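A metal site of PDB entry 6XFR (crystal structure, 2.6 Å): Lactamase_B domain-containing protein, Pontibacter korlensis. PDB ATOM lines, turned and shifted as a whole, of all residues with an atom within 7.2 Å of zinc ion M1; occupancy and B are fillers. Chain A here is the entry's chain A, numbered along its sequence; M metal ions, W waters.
The side-chain carboxylate (OD1) of Asp 82 sits close to the side-chain amino group (NZ) of Lys 83.
A ring nitrogen (ND1) of His 202 is in hydrogen-bond range of the backbone carbonyl oxygen of Pro 32, 2.7 Å away.
The backbone NH (N) of Cys 160 sits at hydrogen-bond distance from the side-chain hydroxyl (OG) of Ser 201.
Residues that only touch zinc ion M1: His 141.
Of the 16 residues printed, 4 come within 4 Å of zinc ion M1.
The nearest printed residue that does not touch zinc ion M1 is His 78 (4.2 Å).
Zinc ion M1 is bound by OD1 of Asp 82, NE2 of His 202 and SG of Cys 160.
Slightly farther from zinc ion M1 lies water W1 (2.7 Å).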
ATOM      1  N   VAL A  31      29.923   0.265 -27.330  1.00  0.00           N
ATOM      2  CA  VAL A  31      28.778  -0.497 -27.826  1.00  0.00           C
ATOM      3  C   VAL A  31      27.556  -0.095 -27.037  1.00  0.00           C
ATOM      4  O   VAL A  31      27.562  -0.148 -25.804  1.00  0.00           O
ATOM      5  CB  VAL A  31      28.989  -2.026 -27.716  1.00  0.00           C
ATOM      6  CG1 VAL A  31      27.741  -2.769 -28.221  1.00  0.00           C
ATOM      7  CG2 VAL A  31      30.244  -2.478 -28.432  1.00  0.00           C
ATOM      8  N   PRO A  32      26.473   0.328 -27.678  1.00  0.00           N
ATOM      9  CA  PRO A  32      25.228   0.511 -26.948  1.00  0.00           C
ATOM     10  C   PRO A  32      24.476  -0.810 -26.787  1.00  0.00           C
ATOM     11  O   PRO A  32      24.629  -1.758 -27.555  1.00  0.00           O
ATOM     12  CB  PRO A  32      24.445   1.460 -27.875  1.00  0.00           C
ATOM     13  CG  PRO A  32      24.878   0.956 -29.292  1.00  0.00           C
ATOM     14  CD  PRO A  32      26.342   0.566 -29.133  1.00  0.00           C
ATOM     15  N   SER A  33      23.627  -0.847 -25.755  1.00  0.00           N
ATOM     16  CA  SER A  33      22.619  -1.883 -25.602  1.00  0.00           C
ATOM     17  C   SER A  33      21.253  -1.217 -25.399  1.00  0.00           C
ATOM     18  O   SER A  33      21.040  -0.524 -24.393  1.00  0.00           O
ATOM     19  CB  SER A  33      22.942  -2.843 -24.458  1.00  0.00           C
ATOM     20  OG  SER A  33      21.999  -3.917 -24.431  1.00  0.00           O
ATOM     21  N   TRP A  51      21.906  -3.051 -18.762  1.00  0.00           N
ATOM     22  CA  TRP A  51      23.084  -3.896 -18.938  1.00  0.00           C
ATOM     23  C   TRP A  51      23.782  -4.079 -17.582  1.00  0.00           C
ATOM     24  O   TRP A  51      24.896  -3.608 -17.352  1.00  0.00           O
ATOM     25  CB  TRP A  51      23.971  -3.249 -19.971  1.00  0.00           C
ATOM     26  CG  TRP A  51      25.013  -4.082 -20.568  1.00  0.00           C
ATOM     27  CD1 TRP A  51      25.466  -5.279 -20.118  1.00  0.00           C
ATOM     28  CD2 TRP A  51      25.756  -3.787 -21.756  1.00  0.00           C
ATOM     29  NE1 TRP A  51      26.451  -5.759 -20.945  1.00  0.00           N
ATOM     30  CE2 TRP A  51      26.653  -4.851 -21.953  1.00  0.00           C
ATOM     31  CE3 TRP A  51      25.757  -2.715 -22.660  1.00  0.00           C
ATOM     32  CZ2 TRP A  51      27.566  -4.873 -23.007  1.00  0.00           C
ATOM     33  CZ3 TRP A  51      26.652  -2.752 -23.720  1.00  0.00           C
ATOM     34  CH2 TRP A  51      27.523  -3.825 -23.894  1.00  0.00           C
ATOM     35  N   HIS A  78      16.626 -12.607 -24.479  1.00  0.00           N
ATOM     36  CA  HIS A  78      17.491 -13.787 -24.416  1.00  0.00           C
ATOM     37  C   HIS A  78      18.347 -13.657 -23.157  1.00  0.00           C
ATOM     38  O   HIS A  78      18.230 -12.682 -22.403  1.00  0.00           O
ATOM     39  CB  HIS A  78      18.266 -13.967 -25.727  1.00  0.00           C
ATOM     40  CG  HIS A  78      19.407 -13.027 -25.927  1.00  0.00           C
ATOM     41  ND1 HIS A  78      19.239 -11.672 -26.058  1.00  0.00           N
ATOM     42  CD2 HIS A  78      20.732 -13.257 -26.073  1.00  0.00           C
ATOM     43  CE1 HIS A  78      20.413 -11.100 -26.256  1.00  0.00           C
ATOM     44  NE2 HIS A  78      21.331 -12.038 -26.273  1.00  0.00           N
ATOM     45  N   HIS A  80      21.602 -13.367 -22.338  1.00  0.00           N
ATOM     46  CA  HIS A  80      22.853 -12.632 -22.149  1.00  0.00           C
ATOM     47  C   HIS A  80      22.657 -11.412 -21.230  1.00  0.00           C
ATOM     48  O   HIS A  80      21.548 -10.881 -21.080  1.00  0.00           O
ATOM     49  CB  HIS A  80      23.450 -12.182 -23.489  1.00  0.00           C
ATOM     50  CG  HIS A  80      24.136 -13.257 -24.270  1.00  0.00           C
ATOM     51  ND1 HIS A  80      24.477 -13.102 -25.605  1.00  0.00           N
ATOM     52  CD2 HIS A  80      24.546 -14.502 -23.924  1.00  0.00           C
ATOM     53  CE1 HIS A  80      25.075 -14.196 -26.039  1.00  0.00           C
ATOM     54  NE2 HIS A  80      25.134 -15.064 -25.039  1.00  0.00           N
ATOM     55  N   ASP A  81      23.774 -10.963 -20.657  1.00  0.00           N
ATOM     56  CA  ASP A  81      23.775  -9.907 -19.641  1.00  0.00           C
ATOM     57  C   ASP A  81      23.189  -8.593 -20.150  1.00  0.00           C
ATOM     58  O   ASP A  81      22.591  -7.844 -19.373  1.00  0.00           O
ATOM     59  CB  ASP A  81      25.216  -9.659 -19.154  1.00  0.00           C
ATOM     60  CG  ASP A  81      25.521 -10.326 -17.821  1.00  0.00           C
ATOM     61  OD1 ASP A  81      24.660 -11.053 -17.250  1.00  0.00           O
ATOM     62  OD2 ASP A  81      26.658 -10.098 -17.334  1.00  0.00           O
ATOM     63  N   ASP A  82      23.396  -8.252 -21.422  1.00  0.00           N
ATOM     64  CA  ASP A  82      22.878  -6.972 -21.890  1.00  0.00           C
ATOM     65  C   ASP A  82      21.360  -6.929 -21.909  1.00  0.00           C
ATOM     66  O   ASP A  82      20.786  -5.858 -21.716  1.00  0.00           O
ATOM     67  CB  ASP A  82      23.461  -6.616 -23.273  1.00  0.00           C
ATOM     68  CG  ASP A  82      23.207  -7.682 -24.329  1.00  0.00           C
ATOM     69  OD1 ASP A  82      22.735  -7.363 -25.446  1.00  0.00           O
ATOM     70  OD2 ASP A  82      23.500  -8.852 -24.054  1.00  0.00           O
ATOM     71  N   LYS A  83      20.683  -8.057 -22.013  1.00  0.00           N
ATOM     72  CA  LYS A  83      19.224  -8.071 -21.972  1.00  0.00           C
ATOM     73  C   LYS A  83      18.654  -8.609 -20.666  1.00  0.00           C
ATOM     74  O   LYS A  83      17.437  -8.487 -20.424  1.00  0.00           O
ATOM     75  CB  LYS A  83      18.662  -8.899 -23.159  1.00  0.00           C
ATOM     76  CG  LYS A  83      19.433  -8.754 -24.506  1.00  0.00           C
ATOM     77  CD  LYS A  83      19.109  -7.471 -25.329  1.00  0.00           C
ATOM     78  CE  LYS A  83      19.982  -6.289 -24.907  1.00  0.00           C
ATOM     79  NZ  LYS A  83      19.825  -4.980 -25.642  1.00  0.00           N
ATOM     80  N   HIS A 141      21.400 -15.076 -33.076  1.00  0.00           N
ATOM     81  CA  HIS A 141      22.444 -14.564 -32.173  1.00  0.00           C
ATOM     82  C   HIS A 141      22.647 -15.524 -30.990  1.00  0.00           C
ATOM     83  O   HIS A 141      23.780 -15.824 -30.598  1.00  0.00           O
ATOM     84  CB  HIS A 141      22.072 -13.143 -31.729  1.00  0.00           C
ATOM     85  CG  HIS A 141      22.797 -12.687 -30.505  1.00  0.00           C
ATOM     86  ND1 HIS A 141      24.146 -12.407 -30.505  1.00  0.00           N
ATOM     87  CD2 HIS A 141      22.371 -12.447 -29.246  1.00  0.00           C
ATOM     88  CE1 HIS A 141      24.514 -12.057 -29.289  1.00  0.00           C
ATOM     89  NE2 HIS A 141      23.457 -12.064 -28.509  1.00  0.00           N
ATOM     90  N   GLY A 159      16.168  -6.945 -30.932  1.00  0.00           N
ATOM     91  CA  GLY A 159      17.268  -7.304 -30.060  1.00  0.00           C
ATOM     92  C   GLY A 159      18.539  -7.614 -30.828  1.00  0.00           C
ATOM     93  O   GLY A 159      18.824  -7.002 -31.868  1.00  0.00           O
ATOM     94  N   CYS A 160      19.310  -8.589 -30.329  1.00  0.00           N
ATOM     95  CA  CYS A 160      20.602  -8.908 -30.933  1.00  0.00           C
ATOM     96  C   CYS A 160      20.516  -9.860 -32.111  1.00  0.00           C
ATOM     97  O   CYS A 160      21.539 -10.173 -32.726  1.00  0.00           O
ATOM     98  CB  CYS A 160      21.543  -9.467 -29.868  1.00  0.00           C
ATOM     99  SG  CYS A 160      21.393  -8.610 -28.295  1.00  0.00           S
ATOM    100  N   LEU A 161      19.299 -10.284 -32.460  1.00  0.00           N
ATOM    101  CA  LEU A 161      19.074 -11.051 -33.678  1.00  0.00           C
ATOM    102  C   LEU A 161      19.261 -10.216 -34.954  1.00  0.00           C
ATOM    103  O   LEU A 161      19.620 -10.755 -36.011  1.00  0.00           O
ATOM    104  CB  LEU A 161      17.654 -11.588 -33.603  1.00  0.00           C
ATOM    105  CG  LEU A 161      17.112 -12.416 -34.750  1.00  0.00           C
ATOM    106  CD1 LEU A 161      17.976 -13.683 -34.942  1.00  0.00           C
ATOM    107  CD2 LEU A 161      15.687 -12.762 -34.423  1.00  0.00           C
ATOM    108  N   ASN A 172      29.319 -10.437 -31.683  1.00  0.00           N
ATOM    109  CA  ASN A 172      29.485 -11.578 -30.797  1.00  0.00           C
ATOM    110  C   ASN A 172      28.729 -12.753 -31.406  1.00  0.00           C
ATOM    111  O   ASN A 172      27.530 -12.660 -31.717  1.00  0.00           O
ATOM    112  CB  ASN A 172      28.965 -11.268 -29.397  1.00  0.00           C
ATOM    113  CG  ASN A 172      29.437 -12.279 -28.362  1.00  0.00           C
ATOM    114  OD1 ASN A 172      30.388 -13.009 -28.600  1.00  0.00           O
ATOM    115  ND2 ASN A 172      28.744 -12.334 -27.238  1.00  0.00           N
ATOM    116  N   SER A 201      19.823  -4.266 -31.168  1.00  0.00           N
ATOM    117  CA  SER A 201      20.310  -4.049 -29.822  1.00  0.00           C
ATOM    118  C   SER A 201      21.515  -3.126 -29.789  1.00  0.00           C
ATOM    119  O   SER A 201      21.619  -2.268 -28.915  1.00  0.00           O
ATOM    120  CB  SER A 201      20.699  -5.399 -29.176  1.00  0.00           C
ATOM    121  OG  SER A 201      19.605  -5.970 -28.514  1.00  0.00           O
ATOM    122  N   HIS A 202      22.410  -3.256 -30.770  1.00  0.00           N
ATOM    123  CA  HIS A 202      23.752  -2.747 -30.592  1.00  0.00           C
ATOM    124  C   HIS A 202      24.111  -1.740 -31.667  1.00  0.00           C
ATOM    125  O   HIS A 202      25.285  -1.532 -31.977  1.00  0.00           O
ATOM    126  CB  HIS A 202      24.761  -3.887 -30.540  1.00  0.00           C
ATOM    127  CG  HIS A 202      24.538  -4.821 -29.397  1.00  0.00           C
ATOM    128  ND1 HIS A 202      24.505  -4.390 -28.083  1.00  0.00           N
ATOM    129  CD2 HIS A 202      24.330  -6.159 -29.360  1.00  0.00           C
ATOM    130  CE1 HIS A 202      24.298  -5.422 -27.291  1.00  0.00           C
ATOM    131  NE2 HIS A 202      24.192  -6.506 -28.036  1.00  0.00           N
HETATM  132 ZN    ZN M   1      23.402  -8.368 -27.170  1.00  0.00          ZN
HETATM  133 ZN    ZN M   2      23.356 -11.517 -26.632  1.00  0.00          ZN
HETATM  134  O   HOH W   1      24.506  -9.055 -29.523  1.00  0.00           O
HETATM  135  O   HOH W   2      26.098 -10.488 -27.142  1.00  0.00           O
